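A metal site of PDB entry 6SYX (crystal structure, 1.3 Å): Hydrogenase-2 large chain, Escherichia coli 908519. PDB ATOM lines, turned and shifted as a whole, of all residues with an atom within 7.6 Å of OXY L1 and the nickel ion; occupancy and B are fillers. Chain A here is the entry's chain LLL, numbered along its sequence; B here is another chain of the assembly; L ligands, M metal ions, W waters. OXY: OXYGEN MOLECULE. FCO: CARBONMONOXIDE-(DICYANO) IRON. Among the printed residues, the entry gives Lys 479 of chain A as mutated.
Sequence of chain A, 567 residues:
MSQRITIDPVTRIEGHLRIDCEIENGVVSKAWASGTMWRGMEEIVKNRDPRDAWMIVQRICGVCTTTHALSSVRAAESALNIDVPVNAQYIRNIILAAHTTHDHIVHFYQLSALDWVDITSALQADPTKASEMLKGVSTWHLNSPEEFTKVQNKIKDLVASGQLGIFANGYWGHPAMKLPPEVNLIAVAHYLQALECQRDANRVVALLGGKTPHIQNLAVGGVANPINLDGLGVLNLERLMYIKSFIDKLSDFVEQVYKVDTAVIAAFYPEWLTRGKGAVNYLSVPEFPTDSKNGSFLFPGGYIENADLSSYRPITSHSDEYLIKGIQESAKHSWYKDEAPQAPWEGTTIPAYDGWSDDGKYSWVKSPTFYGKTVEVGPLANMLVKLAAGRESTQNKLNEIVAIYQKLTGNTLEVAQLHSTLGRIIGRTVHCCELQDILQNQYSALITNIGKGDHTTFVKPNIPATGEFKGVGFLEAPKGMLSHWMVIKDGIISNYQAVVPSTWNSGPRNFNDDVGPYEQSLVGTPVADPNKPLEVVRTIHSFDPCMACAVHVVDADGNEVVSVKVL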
ATOM      1  N   ILE A  13      23.888   9.580  -1.099  1.00  0.00           N
ATOM      2  CA  ILE A  13      23.321   9.750   0.247  1.00  0.00           C
ATOM      3  C   ILE A  13      21.923  10.344   0.085  1.00  0.00           C
ATOM      4  O   ILE A  13      21.515  10.692  -1.064  1.00  0.00           O
ATOM      5  CB  ILE A  13      24.180  10.690   1.124  1.00  0.00           C
ATOM      6  CG1 ILE A  13      24.180  12.123   0.570  1.00  0.00           C
ATOM      7  CG2 ILE A  13      25.573  10.152   1.348  1.00  0.00           C
ATOM      8  CD1 ILE A  13      24.679  13.150   1.564  1.00  0.00           C
ATOM      9  N   GLU A  14      21.194  10.539   1.175  1.00  0.00           N
ATOM     10  CA  GLU A  14      20.029  11.444   1.184  1.00  0.00           C
ATOM     11  C   GLU A  14      20.496  12.870   1.524  1.00  0.00           C
ATOM     12  O   GLU A  14      21.166  13.059   2.591  1.00  0.00           O
ATOM     13  CB  GLU A  14      18.937  10.960   2.161  1.00  0.00           C
ATOM     14  CG  GLU A  14      17.615  11.723   2.011  1.00  0.00           C
ATOM     15  CD  GLU A  14      17.662  13.218   2.287  1.00  0.00           C
ATOM     16  OE1 GLU A  14      18.373  13.618   3.243  1.00  0.00           O
ATOM     17  OE2 GLU A  14      16.908  14.017   1.596  1.00  0.00           O
ATOM     18  N   ILE A  60       9.876  15.183   7.120  1.00  0.00           N
ATOM     19  CA  ILE A  60      11.312  15.369   7.399  1.00  0.00           C
ATOM     20  C   ILE A  60      12.099  14.538   6.365  1.00  0.00           C
ATOM     21  O   ILE A  60      13.178  14.991   5.919  1.00  0.00           O
ATOM     22  CB  ILE A  60      11.663  14.988   8.853  1.00  0.00           C
ATOM     23  CG1 ILE A  60      11.127  16.087   9.799  1.00  0.00           C
ATOM     24  CG2 ILE A  60      13.165  14.755   8.982  1.00  0.00           C
ATOM     25  CD1 ILE A  60      11.215  15.796  11.275  1.00  0.00           C
ATOM     26  N   CYS A  61      11.656  13.325   6.004  1.00  0.00           N
ATOM     27  CA  CYS A  61      12.472  12.451   5.124  1.00  0.00           C
ATOM     28  C   CYS A  61      11.580  11.473   4.347  1.00  0.00           C
ATOM     29  O   CYS A  61      10.740  10.774   4.983  1.00  0.00           O
ATOM     30  CB  CYS A  61      13.553  11.730   5.915  1.00  0.00           C
ATOM     31  SG  CYS A  61      14.736  10.804   4.881  1.00  0.00           S
ATOM     32  N   GLY A  62      11.852  11.332   3.042  1.00  0.00           N
ATOM     33  CA  GLY A  62      11.211  10.328   2.194  1.00  0.00           C
ATOM     34  C   GLY A  62      12.004   9.072   1.956  1.00  0.00           C
ATOM     35  O   GLY A  62      11.435   8.110   1.372  1.00  0.00           O
ATOM     36  N   VAL A  63      13.286   9.025   2.337  1.00  0.00           N
ATOM     37  CA  VAL A  63      14.080   7.778   2.286  1.00  0.00           C
ATOM     38  C   VAL A  63      13.654   6.968   3.522  1.00  0.00           C
ATOM     39  O   VAL A  63      13.088   5.848   3.359  1.00  0.00           O
ATOM     40  CB  VAL A  63      15.595   7.989   2.216  1.00  0.00           C
ATOM     41  CG1 VAL A  63      16.329   6.640   2.261  1.00  0.00           C
ATOM     42  CG2 VAL A  63      15.936   8.765   0.969  1.00  0.00           C
ATOM     43  N   CYS A  64      13.794   7.512   4.725  1.00  0.00           N
ATOM     44  CA  CYS A  64      13.258   6.886   5.968  1.00  0.00           C
ATOM     45  C   CYS A  64      11.835   7.352   6.181  1.00  0.00           C
ATOM     46  O   CYS A  64      11.437   7.749   7.300  1.00  0.00           O
ATOM     47  CB  CYS A  64      14.183   7.084   7.178  1.00  0.00           C
ATOM     48  SG  CYS A  64      14.415   8.813   7.690  1.00  0.00           S
ATOM     49  N   THR A  65      11.002   7.233   5.133  1.00  0.00           N
ATOM     50  CA  THR A  65       9.536   7.363   5.276  1.00  0.00           C
ATOM     51  C   THR A  65       9.042   6.362   6.343  1.00  0.00           C
ATOM     52  O   THR A  65       9.763   5.369   6.641  1.00  0.00           O
ATOM     53  CB  THR A  65       8.863   7.313   3.904  1.00  0.00           C
ATOM     54  OG1 THR A  65       7.494   7.717   4.060  1.00  0.00           O
ATOM     55  CG2 THR A  65       8.921   5.949   3.293  1.00  0.00           C
ATOM     56  N   THR A  67       9.139   6.521   9.496  1.00  0.00           N
ATOM     57  CA  THR A  67       9.823   6.557  10.806  1.00  0.00           C
ATOM     58  C   THR A  67       9.370   7.781  11.615  1.00  0.00           C
ATOM     59  O   THR A  67       9.100   7.677  12.838  1.00  0.00           O
ATOM     60  CB  THR A  67      11.359   6.508  10.672  1.00  0.00           C
ATOM     61  OG1 THR A  67      11.882   7.701  10.099  1.00  0.00           O
ATOM     62  CG2 THR A  67      11.827   5.236   9.977  1.00  0.00           C
ATOM     63  N   HIS A  68       9.363   8.976  11.027  1.00  0.00           N
ATOM     64  CA  HIS A  68       8.995  10.212  11.767  1.00  0.00           C
ATOM     65  C   HIS A  68       7.472  10.220  12.031  1.00  0.00           C
ATOM     66  O   HIS A  68       7.061  10.803  13.061  1.00  0.00           O
ATOM     67  CB  HIS A  68       9.460  11.466  10.965  1.00  0.00           C
ATOM     68  CG  HIS A  68      10.923  11.593  10.863  1.00  0.00           C
ATOM     69  ND1 HIS A  68      11.704  12.021  11.950  1.00  0.00           N
ATOM     70  CD2 HIS A  68      11.758  11.269   9.828  1.00  0.00           C
ATOM     71  CE1 HIS A  68      12.979  11.976  11.553  1.00  0.00           C
ATOM     72  NE2 HIS A  68      13.050  11.507  10.257  1.00  0.00           N
ATOM     73  N   HIS A  99       9.542  -1.689   5.675  1.00  0.00           N
ATOM     74  CA  HIS A  99      10.216  -0.443   5.215  1.00  0.00           C
ATOM     75  C   HIS A  99      11.721  -0.562   5.404  1.00  0.00           C
ATOM     76  O   HIS A  99      12.530  -0.263   4.485  1.00  0.00           O
ATOM     77  CB  HIS A  99       9.718   0.826   5.959  1.00  0.00           C
ATOM     78  CG  HIS A  99      10.620   1.969   5.590  1.00  0.00           C
ATOM     79  ND1 HIS A  99      10.465   2.609   4.387  1.00  0.00           N
ATOM     80  CD2 HIS A  99      11.761   2.413   6.167  1.00  0.00           C
ATOM     81  CE1 HIS A  99      11.500   3.449   4.284  1.00  0.00           C
ATOM     82  NE2 HIS A  99      12.339   3.325   5.310  1.00  0.00           N
ATOM     83  N   ASP A 103      14.988  -0.234   2.867  1.00  0.00           N
ATOM     84  CA  ASP A 103      15.993   0.818   3.109  1.00  0.00           C
ATOM     85  C   ASP A 103      17.409   0.218   3.099  1.00  0.00           C
ATOM     86  O   ASP A 103      18.320   0.725   2.433  1.00  0.00           O
ATOM     87  CB  ASP A 103      15.584   1.473   4.440  1.00  0.00           C
ATOM     88  CG  ASP A 103      16.058   2.824   4.742  1.00  0.00           C
ATOM     89  OD1 ASP A 103      17.335   2.965   4.637  1.00  0.00           O
ATOM     90  OD2 ASP A 103      15.231   3.699   5.255  1.00  0.00           O
ATOM     91  N   LEU A 111      23.329   2.773  -3.196  1.00  0.00           N
ATOM     92  CA  LEU A 111      24.109   3.892  -2.595  1.00  0.00           C
ATOM     93  C   LEU A 111      25.574   3.509  -2.334  1.00  0.00           C
ATOM     94  O   LEU A 111      26.486   4.343  -2.703  1.00  0.00           O
ATOM     95  CB  LEU A 111      23.399   4.447  -1.347  1.00  0.00           C
ATOM     96  CG  LEU A 111      21.920   4.835  -1.528  1.00  0.00           C
ATOM     97  CD1 LEU A 111      21.365   5.385  -0.222  1.00  0.00           C
ATOM     98  CD2 LEU A 111      21.718   5.861  -2.606  1.00  0.00           C
ATOM     99  N   PRO A 478      16.076   2.862  10.687  1.00  0.00           N
ATOM    100  CA  PRO A 478      17.134   2.211   9.933  1.00  0.00           C
ATOM    101  C   PRO A 478      18.534   2.792  10.195  1.00  0.00           C
ATOM    102  O   PRO A 478      19.545   2.056  10.120  1.00  0.00           O
ATOM    103  CB  PRO A 478      16.663   2.401   8.472  1.00  0.00           C
ATOM    104  CG  PRO A 478      15.167   2.452   8.546  1.00  0.00           C
ATOM    105  CD  PRO A 478      14.911   3.213   9.824  1.00  0.00           C
ATOM    106  N   LYS A 479      18.643   4.097  10.452  1.00  0.00           N
ATOM    107  CA  LYS A 479      19.919   4.780  10.722  1.00  0.00           C
ATOM    108  C   LYS A 479      20.210   4.866  12.249  1.00  0.00           C
ATOM    109  O   LYS A 479      21.310   5.346  12.586  1.00  0.00           O
ATOM    110  CB  LYS A 479      19.981   6.179  10.105  1.00  0.00           C
ATOM    111  CG  LYS A 479      20.580   6.274   8.698  1.00  0.00           C
ATOM    112  CD  LYS A 479      19.611   6.461   7.521  1.00  0.00           C
ATOM    113  CE  LYS A 479      18.814   5.232   7.167  1.00  0.00           C
ATOM    114  NZ  LYS A 479      18.601   5.180   5.684  1.00  0.00           N
ATOM    115  N   VAL A 500      17.515  13.209  15.745  1.00  0.00           N
ATOM    116  CA  VAL A 500      17.399  12.166  14.699  1.00  0.00           C
ATOM    117  C   VAL A 500      18.723  11.399  14.607  1.00  0.00           C
ATOM    118  O   VAL A 500      19.799  11.945  14.952  1.00  0.00           O
ATOM    119  CB  VAL A 500      16.978  12.870  13.378  1.00  0.00           C
ATOM    120  CG1 VAL A 500      16.654  11.920  12.251  1.00  0.00           C
ATOM    121  CG2 VAL A 500      15.794  13.788  13.642  1.00  0.00           C
ATOM    122  N   PRO A 501      18.754  10.096  14.217  1.00  0.00           N
ATOM    123  CA  PRO A 501      20.014   9.368  14.271  1.00  0.00           C
ATOM    124  C   PRO A 501      21.166  10.020  13.508  1.00  0.00           C
ATOM    125  O   PRO A 501      22.296  10.096  14.039  1.00  0.00           O
ATOM    126  CB  PRO A 501      19.688   7.926  13.755  1.00  0.00           C
ATOM    127  CG  PRO A 501      18.305   8.036  13.183  1.00  0.00           C
ATOM    128  CD  PRO A 501      17.626   9.192  13.893  1.00  0.00           C
ATOM    129  N   SER A 502      20.953  10.534  12.275  1.00  0.00           N
ATOM    130  CA  SER A 502      22.062  11.203  11.547  1.00  0.00           C
ATOM    131  C   SER A 502      22.475  12.501  12.255  1.00  0.00           C
ATOM    132  O   SER A 502      23.619  12.945  12.044  1.00  0.00           O
ATOM    133  CB  SER A 502      21.735  11.425  10.082  1.00  0.00           C
ATOM    134  OG  SER A 502      21.684  10.205   9.355  1.00  0.00           O
ATOM    135  N   ASP A 544      25.516   5.581   6.388  1.00  0.00           N
ATOM    136  CA  ASP A 544      24.204   5.831   5.696  1.00  0.00           C
ATOM    137  C   ASP A 544      23.688   7.246   5.988  1.00  0.00           C
ATOM    138  O   ASP A 544      22.557   7.472   6.529  1.00  0.00           O
ATOM    139  CB  ASP A 544      23.233   4.709   6.087  1.00  0.00           C
ATOM    140  CG  ASP A 544      21.894   4.621   5.397  1.00  0.00           C
ATOM    141  OD1 ASP A 544      21.661   5.283   4.386  1.00  0.00           O
ATOM    142  OD2 ASP A 544      21.123   3.704   5.863  1.00  0.00           O
ATOM    143  N   PRO A 545      24.431   8.301   5.590  1.00  0.00           N
ATOM    144  CA  PRO A 545      23.984   9.670   5.893  1.00  0.00           C
ATOM    145  C   PRO A 545      22.605  10.038   5.331  1.00  0.00           C
ATOM    146  O   PRO A 545      22.260   9.760   4.174  1.00  0.00           O
ATOM    147  CB  PRO A 545      25.043  10.583   5.272  1.00  0.00           C
ATOM    148  CG  PRO A 545      26.253   9.672   5.142  1.00  0.00           C
ATOM    149  CD  PRO A 545      25.720   8.282   4.843  1.00  0.00           C
ATOM    150  N   CYS A 546      21.840  10.730   6.171  1.00  0.00           N
ATOM    151  CA  CYS A 546      20.526  11.298   5.794  1.00  0.00           C
ATOM    152  C   CYS A 546      20.486  12.746   6.305  1.00  0.00           C
ATOM    153  O   CYS A 546      20.303  12.959   7.515  1.00  0.00           O
ATOM    154  CB  CYS A 546      19.361  10.461   6.322  1.00  0.00           C
ATOM    155  SG  CYS A 546      17.777  11.115   5.689  1.00  0.00           S
ATOM    156  N   MET A 547      20.702  13.725   5.416  1.00  0.00           N
ATOM    157  CA  MET A 547      20.847  15.132   5.904  1.00  0.00           C
ATOM    158  C   MET A 547      19.498  15.867   6.054  1.00  0.00           C
ATOM    159  O   MET A 547      19.417  16.848   6.884  1.00  0.00           O
ATOM    160  CB  MET A 547      21.831  15.935   5.029  1.00  0.00           C
ATOM    161  CG  MET A 547      23.206  15.225   4.896  1.00  0.00           C
ATOM    162  SD  MET A 547      23.946  14.637   6.427  1.00  0.00           S
ATOM    163  CE  MET A 547      24.175  16.209   7.234  1.00  0.00           C
ATOM    164  N   ALA A 548      18.459  15.469   5.313  1.00  0.00           N
ATOM    165  CA  ALA A 548      17.068  15.941   5.581  1.00  0.00           C
ATOM    166  C   ALA A 548      16.709  15.533   7.028  1.00  0.00           C
ATOM    167  O   ALA A 548      16.193  16.344   7.839  1.00  0.00           O
ATOM    168  CB  ALA A 548      16.075  15.427   4.560  1.00  0.00           C
ATOM    169  N   CYS A 549      17.011  14.270   7.383  1.00  0.00           N
ATOM    170  CA  CYS A 549      16.885  13.779   8.772  1.00  0.00           C
ATOM    171  C   CYS A 549      17.767  14.578   9.728  1.00  0.00           C
ATOM    172  O   CYS A 549      17.289  15.014  10.818  1.00  0.00           O
ATOM    173  CB  CYS A 549      17.223  12.299   8.826  1.00  0.00           C
ATOM    174  SG  CYS A 549      15.829  11.226   8.468  1.00  0.00           S
ATOM    175  N   ALA A 550      19.073  14.732   9.430  1.00  0.00           N
ATOM    176  CA  ALA A 550      20.013  15.285  10.428  1.00  0.00           C
ATOM    177  C   ALA A 550      19.588  16.705  10.807  1.00  0.00           C
ATOM    178  O   ALA A 550      19.756  17.082  11.984  1.00  0.00           O
ATOM    179  CB  ALA A 550      21.426  15.313   9.865  1.00  0.00           C
ATOM    180  N   CYS B  21      12.793  16.261   0.476  1.00  0.00           N
ATOM    181  CA  CYS B  21      12.930  15.128   1.441  1.00  0.00           C
ATOM    182  C   CYS B  21      13.400  13.831   0.779  1.00  0.00           C
ATOM    183  O   CYS B  21      13.660  12.872   1.502  1.00  0.00           O
ATOM    184  CB  CYS B  21      11.602  14.912   2.172  1.00  0.00           C
ATOM    185  SG  CYS B  21      10.376  13.922   1.259  1.00  0.00           S
ATOM    186  N   GLU B  26      12.320   8.746  -4.502  1.00  0.00           N
ATOM    187  CA  GLU B  26      11.959   7.409  -4.021  1.00  0.00           C
ATOM    188  C   GLU B  26      10.689   6.859  -4.711  1.00  0.00           C
ATOM    189  O   GLU B  26      10.566   5.617  -4.858  1.00  0.00           O
ATOM    190  CB  GLU B  26      11.789   7.429  -2.487  1.00  0.00           C
ATOM    191  CG  GLU B  26      13.100   7.424  -1.759  1.00  0.00           C
ATOM    192  CD  GLU B  26      13.780   6.077  -1.619  1.00  0.00           C
ATOM    193  OE1 GLU B  26      13.293   5.059  -2.172  1.00  0.00           O
ATOM    194  OE2 GLU B  26      14.939   6.048  -1.000  1.00  0.00           O
HETATM  195  O1  OXY L   1      17.450   7.522   5.179  1.00  0.00           O
HETATM  196  O2  OXY L   1      16.893   8.393   5.785  1.00  0.00           O
HETATM  197 FE   FCO L   2      16.197   9.037   9.081  1.00  0.00          FE
HETATM  198  C1  FCO L   2      17.905   9.412   9.669  1.00  0.00           C
HETATM  199  N1  FCO L   2      19.003   9.650  10.062  1.00  0.00           N
HETATM  200  C2  FCO L   2      16.490   7.204   9.273  1.00  0.00           C
HETATM  201  N2  FCO L   2      16.593   6.038   9.459  1.00  0.00           N
HETATM  202  C3  FCO L   2      15.460   8.968  10.694  1.00  0.00           C
HETATM  203  O3  FCO L   2      14.991   8.909  11.710  1.00  0.00           O
HETATM  204 NI    NI M   1      16.109   9.891   6.585  1.00  0.00          NI
HETATM  205  O   HOH W   1      19.621   7.855   3.313  1.00  0.00           O
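The backbone NH (N) of Cys 64 lies close to an oxygen (O2) of OXY L1, at 3.4 Å.
NZ of Lys 479 lies within hydrogen-bond range of O1 of OXY L1, 2.7 Å away.
The side-chain sulfur (SG) of Cys 64 binds an iron atom (FE) of FCO L2.
The side-chain sulfur (SG) of Cys 549 binds an iron atom (FE) of FCO L2.
The backbone NH of Lys 479 is in hydrogen-bond range of a nitrogen (N2) of FCO L2, at 3.0 Å.
N of Ser 502 sits at hydrogen-bond distance from N1 of FCO L2.
OG of Ser 502 lies within hydrogen-bond range of N1 of FCO L2, at 2.8 Å.
The side-chain carboxylate (OE1) of Glu 14 sits close to the side-chain sulfur (SG) of Cys 546 (3.6 Å).
OG of Ser 502 lies within hydrogen-bond range of N of Cys 546 (3.2 Å).
The side-chain hydroxyl (OG1) of Thr 67 is in hydrogen-bond range of the backbone carbonyl oxygen (O) of Cys 64 (2.8 Å).
A ring nitrogen (NE2) of His 68 lies close to the side-chain sulfur (SG) of Cys 549, at 3.3 Å.
The side-chain sulfur (SG) of Cys 61 sits close to the backbone NH (N) of Val 63.
The side-chain amino group (NZ) of Lys 479 lies within salt-bridge range of the side-chain carboxylate (OD1) of Asp 103, at 2.8 Å.
The side-chain amino group of Lys 479 lies within salt-bridge range of the side-chain carboxylate of Asp 544 (2.9 Å).
The backbone carbonyl oxygen (O) of Val 63 sits close to a ring nitrogen (NE2) of His 99, 3.3 Å away.
Val 63 touches OXY L1.
Hydrophobic or aromatic side chains within 4 Å of OXY L1: Val 63.
Of the 27 residues printed, 5 come within 4 Å of OXY L1.
The nickel ion is bound by an oxygen (O2) of OXY L1 (1.9 Å), the side-chain sulfur of Cys 546 (2.3 Å), the side-chain sulfur of Cys 64 (2.3 Å), the side-chain sulfur of Cys 549 (2.3 Å) and the side-chain sulfur of Cys 61 (2.4 Å).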
